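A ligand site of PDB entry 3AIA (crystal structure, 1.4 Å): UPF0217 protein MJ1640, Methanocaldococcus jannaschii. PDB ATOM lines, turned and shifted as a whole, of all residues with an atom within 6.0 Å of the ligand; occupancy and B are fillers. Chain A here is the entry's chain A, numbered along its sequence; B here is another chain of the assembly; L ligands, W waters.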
ATOM      1  N   TYR A 141     -19.400  13.698   3.866  1.00  0.00           N
ATOM      2  CA  TYR A 141     -19.842  13.784   2.527  1.00  0.00           C
ATOM      3  C   TYR A 141     -21.336  13.559   2.547  1.00  0.00           C
ATOM      4  O   TYR A 141     -21.820  12.443   2.855  1.00  0.00           O
ATOM      5  CB  TYR A 141     -19.069  12.740   1.729  1.00  0.00           C
ATOM      6  CG  TYR A 141     -19.457  12.624   0.306  1.00  0.00           C
ATOM      7  CD1 TYR A 141     -20.007  13.701  -0.392  1.00  0.00           C
ATOM      8  CD2 TYR A 141     -19.278  11.432  -0.364  1.00  0.00           C
ATOM      9  CE1 TYR A 141     -20.353  13.578  -1.737  1.00  0.00           C
ATOM     10  CE2 TYR A 141     -19.612  11.302  -1.712  1.00  0.00           C
ATOM     11  CZ  TYR A 141     -20.150  12.391  -2.385  1.00  0.00           C
ATOM     12  OH  TYR A 141     -20.509  12.268  -3.718  1.00  0.00           O
ATOM     13  N   LEU A 142     -22.068  14.650   2.276  1.00  0.00           N
ATOM     14  CA  LEU A 142     -23.512  14.569   2.174  1.00  0.00           C
ATOM     15  C   LEU A 142     -23.836  13.793   0.908  1.00  0.00           C
ATOM     16  O   LEU A 142     -23.543  14.256  -0.205  1.00  0.00           O
ATOM     17  CB  LEU A 142     -24.166  15.975   2.184  1.00  0.00           C
ATOM     18  CG  LEU A 142     -23.794  16.881   3.380  1.00  0.00           C
ATOM     19  CD1 LEU A 142     -24.456  18.252   3.244  1.00  0.00           C
ATOM     20  CD2 LEU A 142     -24.145  16.254   4.727  1.00  0.00           C
ATOM     21  N   HIS A 143     -24.372  12.598   1.092  1.00  0.00           N
ATOM     22  CA  HIS A 143     -24.728  11.727  -0.022  1.00  0.00           C
ATOM     23  C   HIS A 143     -25.967  10.915   0.342  1.00  0.00           C
ATOM     24  O   HIS A 143     -26.072  10.423   1.469  1.00  0.00           O
ATOM     25  CB  HIS A 143     -23.562  10.792  -0.357  1.00  0.00           C
ATOM     26  CG  HIS A 143     -23.656  10.167  -1.716  1.00  0.00           C
ATOM     27  ND1 HIS A 143     -22.903  10.600  -2.789  1.00  0.00           N
ATOM     28  CD2 HIS A 143     -24.429   9.161  -2.179  1.00  0.00           C
ATOM     29  CE1 HIS A 143     -23.206   9.882  -3.848  1.00  0.00           C
ATOM     30  NE2 HIS A 143     -24.127   9.000  -3.517  1.00  0.00           N
ATOM     31  N   MET A 144     -26.888  10.776  -0.610  1.00  0.00           N
ATOM     32  CA  MET A 144     -28.198  10.126  -0.390  1.00  0.00           C
ATOM     33  C   MET A 144     -28.172   8.771   0.347  1.00  0.00           C
ATOM     34  O   MET A 144     -29.101   8.470   1.101  1.00  0.00           O
ATOM     35  CB  MET A 144     -28.948   9.998  -1.739  1.00  0.00           C
ATOM     36  CG  MET A 144     -30.487  10.077  -1.629  1.00  0.00           C
ATOM     37  SD  MET A 144     -31.396   9.305  -2.967  1.00  0.00           S
ATOM     38  CE  MET A 144     -30.888   7.587  -2.789  1.00  0.00           C
ATOM     39  N   ASN A 145     -27.133   7.971   0.158  1.00  0.00           N
ATOM     40  CA  ASN A 145     -27.096   6.636   0.770  1.00  0.00           C
ATOM     41  C   ASN A 145     -26.157   6.478   1.993  1.00  0.00           C
ATOM     42  O   ASN A 145     -25.818   5.363   2.413  1.00  0.00           O
ATOM     43  CB  ASN A 145     -26.834   5.560  -0.283  1.00  0.00           C
ATOM     44  CG  ASN A 145     -27.916   5.541  -1.378  1.00  0.00           C
ATOM     45  OD1 ASN A 145     -29.071   5.214  -1.115  1.00  0.00           O
ATOM     46  ND2 ASN A 145     -27.532   5.888  -2.591  1.00  0.00           N
ATOM     47  N   ILE A 160     -19.072  18.155   2.348  1.00  0.00           N
ATOM     48  CA  ILE A 160     -18.881  18.137   0.909  1.00  0.00           C
ATOM     49  C   ILE A 160     -20.235  18.023   0.228  1.00  0.00           C
ATOM     50  O   ILE A 160     -21.020  17.110   0.536  1.00  0.00           O
ATOM     51  CB  ILE A 160     -18.041  16.903   0.464  1.00  0.00           C
ATOM     52  CG1 ILE A 160     -16.730  16.801   1.262  1.00  0.00           C
ATOM     53  CG2 ILE A 160     -17.825  16.913  -1.038  1.00  0.00           C
ATOM     54  CD1 ILE A 160     -15.825  17.998   1.140  1.00  0.00           C
ATOM     55  N   ILE A 161     -20.483  18.935  -0.711  1.00  0.00           N
ATOM     56  CA  ILE A 161     -21.739  19.014  -1.438  1.00  0.00           C
ATOM     57  C   ILE A 161     -21.401  19.013  -2.926  1.00  0.00           C
ATOM     58  O   ILE A 161     -20.616  19.835  -3.423  1.00  0.00           O
ATOM     59  CB  ILE A 161     -22.476  20.329  -1.130  1.00  0.00           C
ATOM     60  CG1 ILE A 161     -22.554  20.585   0.380  1.00  0.00           C
ATOM     61  CG2 ILE A 161     -23.846  20.356  -1.765  1.00  0.00           C
ATOM     62  CD1 ILE A 161     -22.424  22.014   0.717  1.00  0.00           C
ATOM     63  N   GLY A 162     -22.015  18.080  -3.648  1.00  0.00           N
ATOM     64  CA  GLY A 162     -21.858  18.043  -5.110  1.00  0.00           C
ATOM     65  C   GLY A 162     -22.876  18.887  -5.840  1.00  0.00           C
ATOM     66  O   GLY A 162     -23.863  19.337  -5.261  1.00  0.00           O
ATOM     67  N   ASP A 163     -22.635  19.093  -7.130  1.00  0.00           N
ATOM     68  CA  ASP A 163     -23.574  19.862  -7.969  1.00  0.00           C
ATOM     69  C   ASP A 163     -24.547  18.902  -8.628  1.00  0.00           C
ATOM     70  O   ASP A 163     -24.692  17.761  -8.182  1.00  0.00           O
ATOM     71  CB  ASP A 163     -22.806  20.765  -8.962  1.00  0.00           C
ATOM     72  CG  ASP A 163     -22.069  19.987 -10.032  1.00  0.00           C
ATOM     73  OD1 ASP A 163     -22.151  18.737 -10.037  1.00  0.00           O
ATOM     74  OD2 ASP A 163     -21.407  20.624 -10.883  1.00  0.00           O
ATOM     75  N   HIS A 164     -25.208  19.319  -9.707  1.00  0.00           N
ATOM     76  CA  HIS A 164     -26.242  18.450 -10.254  1.00  0.00           C
ATOM     77  C   HIS A 164     -25.664  17.123 -10.733  1.00  0.00           C
ATOM     78  O   HIS A 164     -26.266  16.047 -10.545  1.00  0.00           O
ATOM     79  CB  HIS A 164     -26.998  19.100 -11.412  1.00  0.00           C
ATOM     80  CG  HIS A 164     -27.976  18.170 -12.061  1.00  0.00           C
ATOM     81  ND1 HIS A 164     -29.119  17.724 -11.425  1.00  0.00           N
ATOM     82  CD2 HIS A 164     -27.967  17.571 -13.275  1.00  0.00           C
ATOM     83  CE1 HIS A 164     -29.785  16.913 -12.229  1.00  0.00           C
ATOM     84  NE2 HIS A 164     -29.107  16.803 -13.361  1.00  0.00           N
ATOM     85  N   ILE A 165     -24.507  17.199 -11.365  1.00  0.00           N
ATOM     86  CA  ILE A 165     -23.868  15.997 -11.849  1.00  0.00           C
ATOM     87  C   ILE A 165     -23.277  15.202 -10.684  1.00  0.00           C
ATOM     88  O   ILE A 165     -23.311  13.976 -10.685  1.00  0.00           O
ATOM     89  CB  ILE A 165     -22.807  16.335 -12.910  1.00  0.00           C
ATOM     90  CG1 ILE A 165     -23.495  16.871 -14.197  1.00  0.00           C
ATOM     91  CG2 ILE A 165     -21.915  15.125 -13.209  1.00  0.00           C
ATOM     92  CD1 ILE A 165     -24.280  15.815 -15.013  1.00  0.00           C
ATOM     93  N   GLY A 166     -22.734  15.903  -9.695  1.00  0.00           N
ATOM     94  CA  GLY A 166     -22.194  15.257  -8.512  1.00  0.00           C
ATOM     95  C   GLY A 166     -20.684  15.296  -8.481  1.00  0.00           C
ATOM     96  O   GLY A 166     -20.011  15.729  -9.415  1.00  0.00           O
ATOM     97  N   ILE A 167     -20.145  14.789  -7.382  1.00  0.00           N
ATOM     98  CA  ILE A 167     -18.718  14.831  -7.094  1.00  0.00           C
ATOM     99  C   ILE A 167     -17.927  14.007  -8.114  1.00  0.00           C
ATOM    100  O   ILE A 167     -16.822  14.397  -8.518  1.00  0.00           O
ATOM    101  CB  ILE A 167     -18.509  14.326  -5.631  1.00  0.00           C
ATOM    102  CG1 ILE A 167     -19.068  15.336  -4.612  1.00  0.00           C
ATOM    103  CG2 ILE A 167     -17.066  14.017  -5.348  1.00  0.00           C
ATOM    104  CD1 ILE A 167     -18.432  16.735  -4.703  1.00  0.00           C
ATOM    105  N   ILE A 183     -23.165  10.730   4.796  1.00  0.00           N
ATOM    106  CA  ILE A 183     -24.370  11.078   5.562  1.00  0.00           C
ATOM    107  C   ILE A 183     -25.547  11.341   4.634  1.00  0.00           C
ATOM    108  O   ILE A 183     -25.455  12.193   3.727  1.00  0.00           O
ATOM    109  CB  ILE A 183     -24.188  12.374   6.360  1.00  0.00           C
ATOM    110  CG1 ILE A 183     -23.078  12.211   7.418  1.00  0.00           C
ATOM    111  CG2 ILE A 183     -25.523  12.872   6.974  1.00  0.00           C
ATOM    112  CD1 ILE A 183     -22.891  13.467   8.289  1.00  0.00           C
ATOM    113  N   SER A 184     -26.668  10.666   4.898  1.00  0.00           N
ATOM    114  CA  SER A 184     -27.905  10.881   4.167  1.00  0.00           C
ATOM    115  C   SER A 184     -28.830  11.830   4.910  1.00  0.00           C
ATOM    116  O   SER A 184     -28.951  11.764   6.128  1.00  0.00           O
ATOM    117  CB  SER A 184     -28.611   9.559   3.917  1.00  0.00           C
ATOM    118  OG  SER A 184     -29.856   9.822   3.274  1.00  0.00           O
ATOM    119  N   LEU A 185     -29.490  12.700   4.154  1.00  0.00           N
ATOM    120  CA  LEU A 185     -30.362  13.740   4.709  1.00  0.00           C
ATOM    121  C   LEU A 185     -31.830  13.503   4.374  1.00  0.00           C
ATOM    122  O   LEU A 185     -32.691  14.141   4.959  1.00  0.00           O
ATOM    123  CB  LEU A 185     -29.960  15.117   4.153  1.00  0.00           C
ATOM    124  CG  LEU A 185     -28.530  15.593   4.425  1.00  0.00           C
ATOM    125  CD1 LEU A 185     -28.366  16.943   3.722  1.00  0.00           C
ATOM    126  CD2 LEU A 185     -28.198  15.706   5.900  1.00  0.00           C
ATOM    127  N   SER A 186     -32.084  12.618   3.424  1.00  0.00           N
ATOM    128  CA  SER A 186     -33.422  12.452   2.821  1.00  0.00           C
ATOM    129  C   SER A 186     -33.496  11.181   2.000  1.00  0.00           C
ATOM    130  O   SER A 186     -32.481  10.746   1.464  1.00  0.00           O
ATOM    131  CB  SER A 186     -33.702  13.654   1.927  1.00  0.00           C
ATOM    132  OG  SER A 186     -34.930  13.509   1.220  1.00  0.00           O
ATOM    133  N   PRO A 187     -34.685  10.556   1.889  1.00  0.00           N
ATOM    134  CA  PRO A 187     -34.826   9.437   0.955  1.00  0.00           C
ATOM    135  C   PRO A 187     -34.864   9.874  -0.502  1.00  0.00           C
ATOM    136  O   PRO A 187     -34.777   9.043  -1.420  1.00  0.00           O
ATOM    137  CB  PRO A 187     -36.171   8.814   1.333  1.00  0.00           C
ATOM    138  CG  PRO A 187     -36.931   9.920   1.949  1.00  0.00           C
ATOM    139  CD  PRO A 187     -35.932  10.802   2.655  1.00  0.00           C
ATOM    140  N   LEU A 188     -35.015  11.185  -0.729  1.00  0.00           N
ATOM    141  CA  LEU A 188     -35.057  11.701  -2.086  1.00  0.00           C
ATOM    142  C   LEU A 188     -33.753  12.394  -2.454  1.00  0.00           C
ATOM    143  O   LEU A 188     -33.053  12.916  -1.590  1.00  0.00           O
ATOM    144  CB  LEU A 188     -36.216  12.683  -2.281  1.00  0.00           C
ATOM    145  CG  LEU A 188     -37.641  12.166  -2.028  1.00  0.00           C
ATOM    146  CD1 LEU A 188     -38.636  13.307  -2.232  1.00  0.00           C
ATOM    147  CD2 LEU A 188     -37.974  10.970  -2.919  1.00  0.00           C
ATOM    148  N   GLU A 189     -33.439  12.391  -3.741  1.00  0.00           N
ATOM    149  CA  GLU A 189     -32.313  13.155  -4.244  1.00  0.00           C
ATOM    150  C   GLU A 189     -32.698  14.626  -4.401  1.00  0.00           C
ATOM    151  O   GLU A 189     -33.470  14.991  -5.284  1.00  0.00           O
ATOM    152  CB  GLU A 189     -31.808  12.579  -5.562  1.00  0.00           C
ATOM    153  CG  GLU A 189     -30.420  13.054  -5.894  1.00  0.00           C
ATOM    154  CD  GLU A 189     -29.842  12.329  -7.083  1.00  0.00           C
ATOM    155  OE1 GLU A 189     -29.567  11.118  -6.960  1.00  0.00           O
ATOM    156  OE2 GLU A 189     -29.651  12.989  -8.124  1.00  0.00           O
ATOM    157  N   LEU A 190     -32.123  15.454  -3.536  1.00  0.00           N
ATOM    158  CA  LEU A 190     -32.432  16.877  -3.459  1.00  0.00           C
ATOM    159  C   LEU A 190     -31.426  17.729  -4.199  1.00  0.00           C
ATOM    160  O   LEU A 190     -30.308  17.282  -4.504  1.00  0.00           O
ATOM    161  CB  LEU A 190     -32.442  17.317  -1.996  1.00  0.00           C
ATOM    162  CG  LEU A 190     -33.227  16.453  -1.028  1.00  0.00           C
ATOM    163  CD1 LEU A 190     -33.101  17.059   0.335  1.00  0.00           C
ATOM    164  CD2 LEU A 190     -34.692  16.319  -1.449  1.00  0.00           C
ATOM    165  N   HIS A 191     -31.808  18.983  -4.478  1.00  0.00           N
ATOM    166  CA  HIS A 191     -30.847  19.987  -4.924  1.00  0.00           C
ATOM    167  C   HIS A 191     -29.824  20.282  -3.828  1.00  0.00           C
ATOM    168  O   HIS A 191     -30.131  20.218  -2.619  1.00  0.00           O
ATOM    169  CB  HIS A 191     -31.546  21.268  -5.385  1.00  0.00           C
ATOM    170  CG  HIS A 191     -32.156  21.146  -6.754  1.00  0.00           C
ATOM    171  ND1 HIS A 191     -31.627  20.326  -7.732  1.00  0.00           N
ATOM    172  CD2 HIS A 191     -33.218  21.767  -7.322  1.00  0.00           C
ATOM    173  CE1 HIS A 191     -32.347  20.430  -8.826  1.00  0.00           C
ATOM    174  NE2 HIS A 191     -33.316  21.295  -8.611  1.00  0.00           N
ATOM    175  N   ALA A 192     -28.598  20.594  -4.231  1.00  0.00           N
ATOM    176  CA  ALA A 192     -27.504  20.889  -3.315  1.00  0.00           C
ATOM    177  C   ALA A 192     -27.838  21.925  -2.255  1.00  0.00           C
ATOM    178  O   ALA A 192     -27.469  21.789  -1.088  1.00  0.00           O
ATOM    179  CB  ALA A 192     -26.285  21.344  -4.123  1.00  0.00           C
ATOM    180  N   CYS A 195     -29.898  20.639   0.650  1.00  0.00           N
ATOM    181  CA  CYS A 195     -29.082  19.852   1.567  1.00  0.00           C
ATOM    182  C   CYS A 195     -28.417  20.726   2.615  1.00  0.00           C
ATOM    183  O   CYS A 195     -28.337  20.364   3.779  1.00  0.00           O
ATOM    184  CB  CYS A 195     -28.031  19.058   0.803  1.00  0.00           C
ATOM    185  SG  CYS A 195     -28.753  17.807  -0.208  1.00  0.00           S
ATOM    186  N   SER B  49     -33.838  17.036  -7.633  1.00  0.00           N
ATOM    187  CA  SER B  49     -32.723  16.793  -8.527  1.00  0.00           C
ATOM    188  C   SER B  49     -33.162  16.440  -9.944  1.00  0.00           C
ATOM    189  O   SER B  49     -32.676  17.037 -10.899  1.00  0.00           O
ATOM    190  CB  SER B  49     -31.804  15.702  -7.987  1.00  0.00           C
ATOM    191  OG  SER B  49     -30.764  15.457  -8.910  1.00  0.00           O
HETATM  192  C1  LIG L   1     -26.100  15.242  -7.117  1.00  0.00           C
HETATM  193  S1  LIG L   1     -27.346  15.919  -5.980  1.00  0.00           S
HETATM  194  C2  LIG L   1     -26.488  17.396  -5.358  1.00  0.00           C
HETATM  195  C3  LIG L   1     -25.759  17.190  -4.033  1.00  0.00           C
HETATM  196  O1  LIG L   1     -26.690  17.230  -2.980  1.00  0.00           O
HETATM  197  C4  LIG L   1     -25.066  15.834  -3.905  1.00  0.00           C
HETATM  198  O2  LIG L   1     -23.747  15.829  -4.413  1.00  0.00           O
HETATM  199  C5  LIG L   1     -25.068  15.605  -2.418  1.00  0.00           C
HETATM  200  O3  LIG L   1     -23.963  16.279  -1.870  1.00  0.00           O
HETATM  201  C6  LIG L   1     -26.318  16.322  -1.962  1.00  0.00           C
HETATM  202  N1  LIG L   1     -27.509  15.475  -1.720  1.00  0.00           N
HETATM  203  C7  LIG L   1     -28.586  15.334  -2.562  1.00  0.00           C
HETATM  204  N2  LIG L   1     -29.505  14.539  -1.966  1.00  0.00           N
HETATM  205  C8  LIG L   1     -29.015  14.182  -0.744  1.00  0.00           C
HETATM  206  C9  LIG L   1     -29.506  13.390   0.301  1.00  0.00           C
HETATM  207  N3  LIG L   1     -30.694  12.784   0.218  1.00  0.00           N
HETATM  208  N4  LIG L   1     -28.748  13.222   1.429  1.00  0.00           N
HETATM  209  C10 LIG L   1     -27.512  13.831   1.563  1.00  0.00           C
HETATM  210  N5  LIG L   1     -27.017  14.620   0.542  1.00  0.00           N
HETATM  211  C11 LIG L   1     -27.764  14.775  -0.581  1.00  0.00           C
HETATM  212  O   HOH W   1     -22.085  13.895  -5.357  1.00  0.00           O
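The backbone carbonyl oxygen (O) of Leu 142 is in hydrogen-bond range of an oxygen (O3) of the ligand (2.7 Å).
A nitrogen (N4) of the ligand lies within hydrogen-bond range of the backbone NH of Leu 185 (2.9 Å).
The backbone NH (N) of Gly 162 lies within hydrogen-bond range of an oxygen (O2) of the ligand.
The backbone carbonyl oxygen (O) of Leu 188 is in hydrogen-bond range of a nitrogen (N3) of the ligand, 3.0 Å away.
A nitrogen (N3) of the ligand sits at hydrogen-bond distance from the backbone carbonyl oxygen (O) of Ser 186, 3.0 Å away.
An oxygen (O1) of the ligand sits close to the side-chain sulfur (SG) of Cys 195 (3.5 Å).
The backbone NH of Leu 190 lies within hydrogen-bond range of a nitrogen (N2) of the ligand.
N of His 143 lies within hydrogen-bond range of N5 of the ligand, at 3.4 Å.
The side-chain hydroxyl (OG) of Ser 184 sits at hydrogen-bond distance from the backbone carbonyl oxygen (O) of Ser 186 (3.3 Å).
The side-chain sulfur (SG) of Cys 195 lies within hydrogen-bond range of the backbone carbonyl oxygen (O) of His 191 (3.7 Å).
N of Gly 166 sits at hydrogen-bond distance from OD1 of Asp 163 (2.9 Å).
The side-chain carboxylate (OD1) of Asp 163 is in hydrogen-bond range of the backbone NH (N) of Ile 165.
The backbone carbonyl oxygen (O) of Met 144 is in hydrogen-bond range of the side-chain hydroxyl (OG) of Ser 184.
The side-chain sulfur (SD) of Met 144 lies within hydrogen-bond range of the backbone NH (N) of Glu 189, 3.8 Å away.
The backbone carbonyl oxygen of Ile 183 sits at hydrogen-bond distance from the backbone NH of His 143, at 2.9 Å.
The side-chain carboxylate (OE2) of Glu 189 is in hydrogen-bond range of the side-chain hydroxyl (OG) of Ser 49 of chain B (2.8 Å).
Residues that only touch the ligand: Met 144 (3.3 Å), Ile 160 (3.9 Å), Ile 161 (3.6 Å), Asp 163 (3.1 Å), His 164 (3.5 Å), Ile 183 (3.4 Å), Ser 184 (3.7 Å), Glu 189 (3.9 Å) and Ala 192 (3.8 Å).
Hydrophobic or aromatic side chains that line the ligand: Leu 142, Met 144 and Leu 185.
Of the 25 residues printed, 17 come within 4 Å of the ligand.
The nearest printed residue that does not touch the ligand is Gly 166 (4.1 Å).
Water W1 lies within hydrogen-bond range of O2 of the ligand (2.7 Å), OH of Tyr 141 (2.8 Å) and N of Ile 167 (2.9 Å).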
